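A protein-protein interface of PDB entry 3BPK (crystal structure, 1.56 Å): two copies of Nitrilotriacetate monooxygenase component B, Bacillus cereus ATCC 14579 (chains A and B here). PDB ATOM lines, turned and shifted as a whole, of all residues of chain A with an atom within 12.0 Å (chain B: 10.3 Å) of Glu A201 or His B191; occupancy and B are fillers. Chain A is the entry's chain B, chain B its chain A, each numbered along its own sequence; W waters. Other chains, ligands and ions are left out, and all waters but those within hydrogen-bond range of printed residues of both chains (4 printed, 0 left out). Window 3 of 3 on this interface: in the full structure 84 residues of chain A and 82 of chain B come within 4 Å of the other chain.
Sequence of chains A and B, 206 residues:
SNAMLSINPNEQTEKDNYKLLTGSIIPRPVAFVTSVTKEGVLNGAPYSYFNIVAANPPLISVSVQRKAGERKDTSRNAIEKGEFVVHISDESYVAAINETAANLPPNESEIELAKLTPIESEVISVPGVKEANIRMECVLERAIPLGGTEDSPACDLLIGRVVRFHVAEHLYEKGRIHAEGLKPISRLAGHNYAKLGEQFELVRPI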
ATOM      1  N   ARG A 176     -18.195  11.255  32.184  1.00  0.00           N
ATOM      2  CA  ARG A 176     -19.453  10.956  31.541  1.00  0.00           C
ATOM      3  C   ARG A 176     -20.476  10.473  32.556  1.00  0.00           C
ATOM      4  O   ARG A 176     -20.139  10.115  33.676  1.00  0.00           O
ATOM      5  CB  ARG A 176     -19.254   9.913  30.433  1.00  0.00           C
ATOM      6  CG  ARG A 176     -18.221  10.391  29.377  1.00  0.00           C
ATOM      7  CD  ARG A 176     -18.249   9.569  28.129  1.00  0.00           C
ATOM      8  NE  ARG A 176     -18.040  10.435  26.954  1.00  0.00           N
ATOM      9  CZ  ARG A 176     -16.862  10.821  26.470  1.00  0.00           C
ATOM     10  NH1 ARG A 176     -15.724  10.431  27.041  1.00  0.00           N
ATOM     11  NH2 ARG A 176     -16.835  11.605  25.402  1.00  0.00           N
ATOM     12  N   ILE A 177     -21.742  10.518  32.149  1.00  0.00           N
ATOM     13  CA  ILE A 177     -22.867  10.115  32.997  1.00  0.00           C
ATOM     14  C   ILE A 177     -23.460   8.819  32.485  1.00  0.00           C
ATOM     15  O   ILE A 177     -23.735   8.718  31.284  1.00  0.00           O
ATOM     16  CB  ILE A 177     -23.996  11.223  32.986  1.00  0.00           C
ATOM     17  CG1 ILE A 177     -23.455  12.564  33.501  1.00  0.00           C
ATOM     18  CG2 ILE A 177     -25.223  10.779  33.762  1.00  0.00           C
ATOM     19  CD1 ILE A 177     -22.949  12.522  34.947  1.00  0.00           C
ATOM     20  N   ALA A 179     -26.237   6.882  31.574  1.00  0.00           N
ATOM     21  CA  ALA A 179     -27.641   7.173  31.280  1.00  0.00           C
ATOM     22  C   ALA A 179     -28.590   6.127  31.872  1.00  0.00           C
ATOM     23  O   ALA A 179     -29.631   6.481  32.445  1.00  0.00           O
ATOM     24  CB  ALA A 179     -27.838   7.303  29.749  1.00  0.00           C
ATOM     25  N   LEU A 196     -36.404   6.388  29.733  1.00  0.00           N
ATOM     26  CA  LEU A 196     -35.376   6.478  28.722  1.00  0.00           C
ATOM     27  C   LEU A 196     -35.555   5.302  27.764  1.00  0.00           C
ATOM     28  O   LEU A 196     -35.701   4.145  28.202  1.00  0.00           O
ATOM     29  CB  LEU A 196     -33.972   6.436  29.362  1.00  0.00           C
ATOM     30  CG  LEU A 196     -32.783   6.610  28.397  1.00  0.00           C
ATOM     31  CD1 LEU A 196     -32.814   7.972  27.664  1.00  0.00           C
ATOM     32  CD2 LEU A 196     -31.485   6.412  29.155  1.00  0.00           C
ATOM     33  N   GLY A 197     -35.547   5.573  26.465  1.00  0.00           N
ATOM     34  CA  GLY A 197     -35.710   4.492  25.485  1.00  0.00           C
ATOM     35  C   GLY A 197     -34.448   3.710  25.144  1.00  0.00           C
ATOM     36  O   GLY A 197     -33.344   3.987  25.652  1.00  0.00           O
ATOM     37  N   GLU A 198     -34.633   2.734  24.261  1.00  0.00           N
ATOM     38  CA  GLU A 198     -33.525   1.895  23.825  1.00  0.00           C
ATOM     39  C   GLU A 198     -32.484   2.721  23.114  1.00  0.00           C
ATOM     40  O   GLU A 198     -32.788   3.539  22.254  1.00  0.00           O
ATOM     41  CB  GLU A 198     -34.011   0.778  22.908  1.00  0.00           C
ATOM     42  CG  GLU A 198     -32.871   0.043  22.251  1.00  0.00           C
ATOM     43  CD  GLU A 198     -33.320  -1.060  21.323  1.00  0.00           C
ATOM     44  OE1 GLU A 198     -34.016  -0.774  20.304  1.00  0.00           O
ATOM     45  OE2 GLU A 198     -32.947  -2.218  21.610  1.00  0.00           O
ATOM     46  N   GLN A 199     -31.231   2.516  23.490  1.00  0.00           N
ATOM     47  CA  GLN A 199     -30.156   3.286  22.899  1.00  0.00           C
ATOM     48  C   GLN A 199     -29.664   2.685  21.582  1.00  0.00           C
ATOM     49  O   GLN A 199     -29.786   1.472  21.327  1.00  0.00           O
ATOM     50  CB  GLN A 199     -29.005   3.426  23.890  1.00  0.00           C
ATOM     51  CG  GLN A 199     -29.403   4.175  25.169  1.00  0.00           C
ATOM     52  CD  GLN A 199     -28.200   4.402  26.058  1.00  0.00           C
ATOM     53  OE1 GLN A 199     -27.130   4.799  25.578  1.00  0.00           O
ATOM     54  NE2 GLN A 199     -28.365   4.165  27.364  1.00  0.00           N
ATOM     55  N   PHE A 200     -29.106   3.546  20.743  1.00  0.00           N
ATOM     56  CA  PHE A 200     -28.402   3.124  19.552  1.00  0.00           C
ATOM     57  C   PHE A 200     -27.324   4.132  19.232  1.00  0.00           C
ATOM     58  O   PHE A 200     -27.370   5.290  19.691  1.00  0.00           O
ATOM     59  CB  PHE A 200     -29.352   2.893  18.365  1.00  0.00           C
ATOM     60  CG  PHE A 200     -30.084   4.134  17.889  1.00  0.00           C
ATOM     61  CD1 PHE A 200     -29.588   4.898  16.817  1.00  0.00           C
ATOM     62  CD2 PHE A 200     -31.278   4.507  18.479  1.00  0.00           C
ATOM     63  CE1 PHE A 200     -30.288   6.059  16.352  1.00  0.00           C
ATOM     64  CE2 PHE A 200     -31.970   5.654  18.026  1.00  0.00           C
ATOM     65  CZ  PHE A 200     -31.477   6.421  16.960  1.00  0.00           C
ATOM     66  N   GLU A 201     -26.345   3.682  18.460  1.00  0.00           N
ATOM     67  CA  GLU A 201     -25.212   4.511  18.073  1.00  0.00           C
ATOM     68  C   GLU A 201     -25.188   4.649  16.568  1.00  0.00           C
ATOM     69  O   GLU A 201     -25.517   3.696  15.857  1.00  0.00           O
ATOM     70  CB  GLU A 201     -23.886   3.871  18.497  1.00  0.00           C
ATOM     71  CG  GLU A 201     -23.802   3.410  19.929  1.00  0.00           C
ATOM     72  CD  GLU A 201     -22.515   2.653  20.206  1.00  0.00           C
ATOM     73  OE1 GLU A 201     -22.597   1.531  20.745  1.00  0.00           O
ATOM     74  OE2 GLU A 201     -21.426   3.180  19.877  1.00  0.00           O
ATOM     75  N   LEU A 202     -24.789   5.830  16.099  1.00  0.00           N
ATOM     76  CA  LEU A 202     -24.602   6.035  14.670  1.00  0.00           C
ATOM     77  C   LEU A 202     -23.166   6.439  14.338  1.00  0.00           C
ATOM     78  O   LEU A 202     -22.521   7.185  15.076  1.00  0.00           O
ATOM     79  CB  LEU A 202     -25.621   7.050  14.111  1.00  0.00           C
ATOM     80  CG  LEU A 202     -26.809   6.493  13.311  1.00  0.00           C
ATOM     81  CD1 LEU A 202     -27.521   5.369  14.026  1.00  0.00           C
ATOM     82  CD2 LEU A 202     -27.809   7.585  13.002  1.00  0.00           C
ATOM     83  N   TYR B  18     -18.948  20.295  28.503  1.00  0.00           N
ATOM     84  CA  TYR B  18     -19.740  19.725  27.413  1.00  0.00           C
ATOM     85  C   TYR B  18     -20.193  18.284  27.709  1.00  0.00           C
ATOM     86  O   TYR B  18     -21.374  17.939  27.569  1.00  0.00           O
ATOM     87  CB  TYR B  18     -18.945  19.755  26.106  1.00  0.00           C
ATOM     88  CG  TYR B  18     -19.604  19.051  24.956  1.00  0.00           C
ATOM     89  CD1 TYR B  18     -20.563  19.704  24.178  1.00  0.00           C
ATOM     90  CD2 TYR B  18     -19.274  17.733  24.633  1.00  0.00           C
ATOM     91  CE1 TYR B  18     -21.163  19.071  23.091  1.00  0.00           C
ATOM     92  CE2 TYR B  18     -19.882  17.075  23.545  1.00  0.00           C
ATOM     93  CZ  TYR B  18     -20.848  17.758  22.790  1.00  0.00           C
ATOM     94  OH  TYR B  18     -21.508  17.138  21.719  1.00  0.00           O
ATOM     95  N   LYS B  19     -19.249  17.448  28.147  1.00  0.00           N
ATOM     96  CA  LYS B  19     -19.580  16.080  28.503  1.00  0.00           C
ATOM     97  C   LYS B  19     -20.628  16.007  29.627  1.00  0.00           C
ATOM     98  O   LYS B  19     -21.532  15.172  29.543  1.00  0.00           O
ATOM     99  CB  LYS B  19     -18.309  15.297  28.904  1.00  0.00           C
ATOM    100  CG  LYS B  19     -17.444  14.974  27.702  1.00  0.00           C
ATOM    101  CD  LYS B  19     -15.997  14.542  28.085  1.00  0.00           C
ATOM    102  CE  LYS B  19     -15.964  13.314  28.984  1.00  0.00           C
ATOM    103  NZ  LYS B  19     -14.510  12.917  29.273  1.00  0.00           N
ATOM    104  N   THR B  22     -24.187  17.362  28.238  1.00  0.00           N
ATOM    105  CA  THR B  22     -24.815  16.462  27.277  1.00  0.00           C
ATOM    106  C   THR B  22     -25.149  15.079  27.829  1.00  0.00           C
ATOM    107  O   THR B  22     -25.986  14.365  27.246  1.00  0.00           O
ATOM    108  CB  THR B  22     -23.972  16.335  25.977  1.00  0.00           C
ATOM    109  OG1 THR B  22     -22.668  15.817  26.290  1.00  0.00           O
ATOM    110  CG2 THR B  22     -23.843  17.667  25.241  1.00  0.00           C
ATOM    111  N   GLY B  23     -24.478  14.682  28.917  1.00  0.00           N
ATOM    112  CA  GLY B  23     -24.798  13.391  29.552  1.00  0.00           C
ATOM    113  C   GLY B  23     -25.863  13.497  30.629  1.00  0.00           C
ATOM    114  O   GLY B  23     -26.499  12.483  30.966  1.00  0.00           O
ATOM    115  N   ARG B  28     -32.648  14.417  24.622  1.00  0.00           N
ATOM    116  CA  ARG B  28     -32.941  15.677  23.912  1.00  0.00           C
ATOM    117  C   ARG B  28     -33.544  15.417  22.548  1.00  0.00           C
ATOM    118  O   ARG B  28     -32.987  14.674  21.753  1.00  0.00           O
ATOM    119  CB  ARG B  28     -31.645  16.467  23.727  1.00  0.00           C
ATOM    120  CG  ARG B  28     -31.033  16.934  25.062  1.00  0.00           C
ATOM    121  CD  ARG B  28     -29.779  17.825  24.825  1.00  0.00           C
ATOM    122  NE  ARG B  28     -28.739  17.197  23.990  1.00  0.00           N
ATOM    123  CZ  ARG B  28     -27.899  16.244  24.418  1.00  0.00           C
ATOM    124  NH1 ARG B  28     -27.980  15.776  25.685  1.00  0.00           N
ATOM    125  NH2 ARG B  28     -26.954  15.756  23.587  1.00  0.00           N
ATOM    126  N   VAL B  30     -34.381  15.980  18.645  1.00  0.00           N
ATOM    127  CA  VAL B  30     -33.433  16.434  17.609  1.00  0.00           C
ATOM    128  C   VAL B  30     -34.183  17.144  16.481  1.00  0.00           C
ATOM    129  O   VAL B  30     -35.036  16.523  15.845  1.00  0.00           O
ATOM    130  CB  VAL B  30     -32.611  15.252  17.046  1.00  0.00           C
ATOM    131  CG1 VAL B  30     -31.719  15.698  15.896  1.00  0.00           C
ATOM    132  CG2 VAL B  30     -31.785  14.583  18.170  1.00  0.00           C
ATOM    133  N   SER B  48     -29.647  19.124  18.587  1.00  0.00           N
ATOM    134  CA  SER B  48     -30.402  18.585  19.712  1.00  0.00           C
ATOM    135  C   SER B  48     -30.665  19.600  20.837  1.00  0.00           C
ATOM    136  O   SER B  48     -31.376  19.277  21.782  1.00  0.00           O
ATOM    137  CB  SER B  48     -29.704  17.365  20.309  1.00  0.00           C
ATOM    138  OG  SER B  48     -28.571  17.727  21.087  1.00  0.00           O
ATOM    139  N   VAL B  94     -33.530   8.873  10.413  1.00  0.00           N
ATOM    140  CA  VAL B  94     -32.359   9.283  11.194  1.00  0.00           C
ATOM    141  C   VAL B  94     -31.008   8.947  10.501  1.00  0.00           C
ATOM    142  O   VAL B  94     -30.040   9.692  10.615  1.00  0.00           O
ATOM    143  CB  VAL B  94     -32.413   8.760  12.666  1.00  0.00           C
ATOM    144  CG1 VAL B  94     -32.293   7.225  12.699  1.00  0.00           C
ATOM    145  CG2 VAL B  94     -31.348   9.475  13.526  1.00  0.00           C
ATOM    146  N   ALA B  95     -30.944   7.832   9.775  1.00  0.00           N
ATOM    147  CA  ALA B  95     -29.722   7.498   9.051  1.00  0.00           C
ATOM    148  C   ALA B  95     -29.320   8.620   8.071  1.00  0.00           C
ATOM    149  O   ALA B  95     -28.156   9.037   8.025  1.00  0.00           O
ATOM    150  CB  ALA B  95     -29.895   6.162   8.314  1.00  0.00           C
ATOM    151  N   ASN B  98     -28.277  11.787  10.048  1.00  0.00           N
ATOM    152  CA  ASN B  98     -26.894  11.638  10.472  1.00  0.00           C
ATOM    153  C   ASN B  98     -25.865  11.926   9.359  1.00  0.00           C
ATOM    154  O   ASN B  98     -24.818  12.518   9.624  1.00  0.00           O
ATOM    155  CB  ASN B  98     -26.676  10.242  11.069  1.00  0.00           C
ATOM    156  CG  ASN B  98     -25.355  10.128  11.842  1.00  0.00           C
ATOM    157  OD1 ASN B  98     -24.508   9.316  11.491  1.00  0.00           O
ATOM    158  ND2 ASN B  98     -25.191  10.924  12.903  1.00  0.00           N
ATOM    159  N   ALA B 101     -24.722  15.652   9.111  1.00  0.00           N
ATOM    160  CA  ALA B 101     -23.923  16.295  10.161  1.00  0.00           C
ATOM    161  C   ALA B 101     -22.517  16.634   9.637  1.00  0.00           C
ATOM    162  O   ALA B 101     -21.870  17.581  10.110  1.00  0.00           O
ATOM    163  CB  ALA B 101     -23.859  15.441  11.415  1.00  0.00           C
ATOM    164  N   ILE B 185     -36.665  10.323  17.508  1.00  0.00           N
ATOM    165  CA  ILE B 185     -35.359  10.012  18.079  1.00  0.00           C
ATOM    166  C   ILE B 185     -34.811  11.166  18.892  1.00  0.00           C
ATOM    167  O   ILE B 185     -35.087  12.346  18.622  1.00  0.00           O
ATOM    168  CB  ILE B 185     -34.340   9.468  17.066  1.00  0.00           C
ATOM    169  CG1 ILE B 185     -33.966  10.520  16.031  1.00  0.00           C
ATOM    170  CG2 ILE B 185     -34.869   8.165  16.394  1.00  0.00           C
ATOM    171  CD1 ILE B 185     -32.865  11.435  16.411  1.00  0.00           C
ATOM    172  N   SER B 186     -34.003  10.781  19.877  1.00  0.00           N
ATOM    173  CA  SER B 186     -33.438  11.731  20.823  1.00  0.00           C
ATOM    174  C   SER B 186     -31.931  11.528  20.915  1.00  0.00           C
ATOM    175  O   SER B 186     -31.416  10.452  20.608  1.00  0.00           O
ATOM    176  CB  SER B 186     -34.114  11.594  22.197  1.00  0.00           C
ATOM    177  OG  SER B 186     -34.021  10.266  22.697  1.00  0.00           O
ATOM    178  N   ARG B 187     -31.233  12.580  21.325  1.00  0.00           N
ATOM    179  CA  ARG B 187     -29.795  12.530  21.492  1.00  0.00           C
ATOM    180  C   ARG B 187     -29.440  12.394  22.972  1.00  0.00           C
ATOM    181  O   ARG B 187     -30.071  13.020  23.859  1.00  0.00           O
ATOM    182  CB  ARG B 187     -29.161  13.813  20.923  1.00  0.00           C
ATOM    183  CG  ARG B 187     -27.638  13.822  20.822  1.00  0.00           C
ATOM    184  CD  ARG B 187     -27.127  13.124  19.556  1.00  0.00           C
ATOM    185  NE  ARG B 187     -25.663  13.110  19.476  1.00  0.00           N
ATOM    186  CZ  ARG B 187     -24.892  14.071  18.955  1.00  0.00           C
ATOM    187  NH1 ARG B 187     -25.416  15.185  18.425  1.00  0.00           N
ATOM    188  NH2 ARG B 187     -23.571  13.911  18.960  1.00  0.00           N
ATOM    189  N   LEU B 188     -28.437  11.552  23.225  1.00  0.00           N
ATOM    190  CA  LEU B 188     -27.807  11.476  24.537  1.00  0.00           C
ATOM    191  C   LEU B 188     -26.376  12.043  24.460  1.00  0.00           C
ATOM    192  O   LEU B 188     -26.136  12.982  23.737  1.00  0.00           O
ATOM    193  CB  LEU B 188     -27.834  10.023  25.050  1.00  0.00           C
ATOM    194  CG  LEU B 188     -29.184   9.301  24.940  1.00  0.00           C
ATOM    195  CD1 LEU B 188     -29.034   7.867  25.420  1.00  0.00           C
ATOM    196  CD2 LEU B 188     -30.347  10.023  25.647  1.00  0.00           C
ATOM    197  N   ALA B 189     -25.425  11.490  25.220  1.00  0.00           N
ATOM    198  CA  ALA B 189     -24.069  11.989  25.163  1.00  0.00           C
ATOM    199  C   ALA B 189     -23.297  11.252  24.081  1.00  0.00           C
ATOM    200  O   ALA B 189     -23.732  10.188  23.627  1.00  0.00           O
ATOM    201  CB  ALA B 189     -23.387  11.793  26.528  1.00  0.00           C
ATOM    202  N   GLY B 190     -22.148  11.791  23.679  1.00  0.00           N
ATOM    203  CA  GLY B 190     -21.343  11.125  22.632  1.00  0.00           C
ATOM    204  C   GLY B 190     -22.137  10.944  21.345  1.00  0.00           C
ATOM    205  O   GLY B 190     -22.938  11.804  20.977  1.00  0.00           O
ATOM    206  N   HIS B 191     -21.952   9.800  20.673  1.00  0.00           N
ATOM    207  CA  HIS B 191     -22.740   9.481  19.477  1.00  0.00           C
ATOM    208  C   HIS B 191     -23.924   8.587  19.829  1.00  0.00           C
ATOM    209  O   HIS B 191     -24.386   7.792  19.001  1.00  0.00           O
ATOM    210  CB  HIS B 191     -21.876   8.814  18.392  1.00  0.00           C
ATOM    211  CG  HIS B 191     -21.137   7.594  18.857  1.00  0.00           C
ATOM    212  ND1 HIS B 191     -19.979   7.151  18.249  1.00  0.00           N
ATOM    213  CD2 HIS B 191     -21.385   6.726  19.870  1.00  0.00           C
ATOM    214  CE1 HIS B 191     -19.549   6.063  18.866  1.00  0.00           C
ATOM    215  NE2 HIS B 191     -20.383   5.785  19.853  1.00  0.00           N
ATOM    216  N   ASN B 192     -24.422   8.721  21.059  1.00  0.00           N
ATOM    217  CA  ASN B 192     -25.515   7.894  21.495  1.00  0.00           C
ATOM    218  C   ASN B 192     -26.848   8.579  21.279  1.00  0.00           C
ATOM    219  O   ASN B 192     -26.966   9.785  21.483  1.00  0.00           O
ATOM    220  CB  ASN B 192     -25.345   7.517  22.949  1.00  0.00           C
ATOM    221  CG  ASN B 192     -24.053   6.795  23.176  1.00  0.00           C
ATOM    222  OD1 ASN B 192     -23.900   5.676  22.715  1.00  0.00           O
ATOM    223  ND2 ASN B 192     -23.087   7.459  23.820  1.00  0.00           N
ATOM    224  N   TYR B 193     -27.812   7.772  20.856  1.00  0.00           N
ATOM    225  CA  TYR B 193     -29.194   8.207  20.658  1.00  0.00           C
ATOM    226  C   TYR B 193     -30.129   7.287  21.394  1.00  0.00           C
ATOM    227  O   TYR B 193     -29.730   6.209  21.827  1.00  0.00           O
ATOM    228  CB  TYR B 193     -29.524   8.206  19.166  1.00  0.00           C
ATOM    229  CG  TYR B 193     -28.716   9.221  18.425  1.00  0.00           C
ATOM    230  CD1 TYR B 193     -29.299  10.409  17.989  1.00  0.00           C
ATOM    231  CD2 TYR B 193     -27.359   9.019  18.179  1.00  0.00           C
ATOM    232  CE1 TYR B 193     -28.552  11.345  17.306  1.00  0.00           C
ATOM    233  CE2 TYR B 193     -26.614   9.948  17.514  1.00  0.00           C
ATOM    234  CZ  TYR B 193     -27.213  11.110  17.091  1.00  0.00           C
ATOM    235  OH  TYR B 193     -26.453  12.033  16.437  1.00  0.00           O
ATOM    236  N   ALA B 194     -31.379   7.701  21.542  1.00  0.00           N
ATOM    237  CA  ALA B 194     -32.383   6.838  22.124  1.00  0.00           C
ATOM    238  C   ALA B 194     -33.665   6.899  21.307  1.00  0.00           C
ATOM    239  O   ALA B 194     -34.054   7.958  20.825  1.00  0.00           O
ATOM    240  CB  ALA B 194     -32.672   7.211  23.541  1.00  0.00           C
ATOM    241  N   LYS B 195     -34.292   5.734  21.148  1.00  0.00           N
ATOM    242  CA  LYS B 195     -35.670   5.654  20.709  1.00  0.00           C
ATOM    243  C   LYS B 195     -36.601   6.164  21.809  1.00  0.00           C
ATOM    244  O   LYS B 195     -36.177   6.390  22.967  1.00  0.00           O
ATOM    245  CB  LYS B 195     -35.990   4.183  20.368  1.00  0.00           C
ATOM    246  CG  LYS B 195     -35.107   3.679  19.240  1.00  0.00           C
ATOM    247  CD  LYS B 195     -35.435   2.230  18.861  1.00  0.00           C
ATOM    248  CE  LYS B 195     -34.427   1.755  17.837  1.00  0.00           C
ATOM    249  NZ  LYS B 195     -34.708   0.302  17.523  1.00  0.00           N
HETATM  250  O   HOH W   1     -21.821   9.117  13.159  1.00  0.00           O
HETATM  251  O   HOH W   2     -35.568   8.328  24.954  1.00  0.00           O
HETATM  252  O   HOH W   3     -25.694  10.109  29.850  1.00  0.00           O
HETATM  253  O   HOH W   4     -20.551   9.381  25.425  1.00  0.00           O
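The side-chain carboxylate (OE2) of Glu A201 sits at hydrogen-bond distance from a ring nitrogen (NE2) of His B191. N of Tyr B193 is in hydrogen-bond range of O of Phe A200 (2.8 Å). OE1 of Glu A198 lies within salt-bridge range of NZ of Lys B195, at 3.1 Å.
NH2 of Arg B28 sits at hydrogen-bond distance from O of Leu B188 (2.9 Å). The backbone NH (N) of Ala B194 is in hydrogen-bond range of the backbone carbonyl oxygen (O) of Ser B186 (2.9 Å). OH of Tyr B193 sits at hydrogen-bond distance from NE of Arg B187, at 3.3 Å. The side-chain amide nitrogen (ND2) of Asn B192 lies within hydrogen-bond range of the backbone carbonyl oxygen (O) of Ala B189, 2.8 Å away.
Ile A177 touches Gly B23 (CB to O, 3.5 Å). CD1 of Leu A196 touches CD2 of Leu B188 (3.8 Å). CB of Ala B194 touches O of Gly A197, at 3.9 Å. CD1 of Leu B188 touches OE1 of Gln A199, 3.6 Å away. O of Tyr B193 touches CA of Gln A199, at 3.1 Å. Phe A200 touches His B191. Phe A200 touches Asn B192. Phe A200 touches Ala B194 (CE2 to C, 3.9 Å). Lys B195 touches Phe A200. Glu A201 touches Asn B192 (CG to OD1, 3.6 Å).
Printed residues of chain B within 4 Å of Glu A201: His B191 (2.8 Å) and Asn B192 (3.6 Å). Printed residues of chain A within 4 Å of His B191: Phe A200 (3.95 Å), Glu A201 (2.8 Å) and Leu A202 (3.5 Å). Gly B190 touches none of the printed residues of chain A. Of the printed residues of chain B, Phe A200 touches Ile B185, His B191, Asn B192, Tyr B193, Ala B194 and Lys B195. Printed residues of chain A within 4 Å of Tyr B193: Gln A199 (3.1 Å) and Phe A200 (2.8 Å). Printed residues of chain B within 4 Å of Glu A198: Ala B194 and Lys B195. Printed residues of chain A within 4 Å of Val B94: Leu A202. Thr B22 touches none of the printed residues of chain A. Val B30 touches none of the printed residues of chain A. The nearest printed residue of chain B that does not touch Glu A201 is Tyr B193 (5.0 Å). The nearest printed residue of chain A that does not touch His B191 is Arg A176 (7.2 Å). The nearest printed residue of chain A that does not touch Lys B195 is Leu A196 (5.0 Å).
Printed residues of chain B that touch a printed residue of chain A: Lys B19, Gly B23, Val B94, Asn B98, Ile B185, Leu B188, His B191, Asn B192, Tyr B193, Ala B194 and Lys B195. Hydrophobic or aromatic side chains of chain B within 4 Å of the printed part of chain A: Ile B185, Leu B188, His B191, Tyr B193 and Ala B194. Of the 10 printed residues of chain A, 9 touch a printed residue of chain B. Printed residues of chain A that touch a printed residue of chain B: Arg A176, Ile A177, Leu A196, Gly A197, Glu A198, Gln A199, Phe A200, Glu A201 and Leu A202. Among the printed residues, Asp or Glu carboxylates within 4 Å of a Lys or Arg side-chain nitrogen of the other chain: Glu A198 with Lys B195 (3.1 Å).
No position is printed for both chains. Of the 20 pairs that touch across the chains among the printed residues, none has its exchanged pair printed and touching as well.
Water W3 bridges the backbone carbonyl oxygen of Gly B23 and the backbone carbonyl oxygen of Ile A177. Water W1 bridges the backbone carbonyl oxygen of Leu A202 and the side-chain amide oxygen of Asn B98. Water W2 lies within hydrogen-bond range of O of Lys B195 (2.8 Å), N of Gly A197 (3.1 Å) and OG of Ser B186 (3.4 Å). Water W4 bridges the guanidinium group of Arg A176 and the backbone NH of Gly B190.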
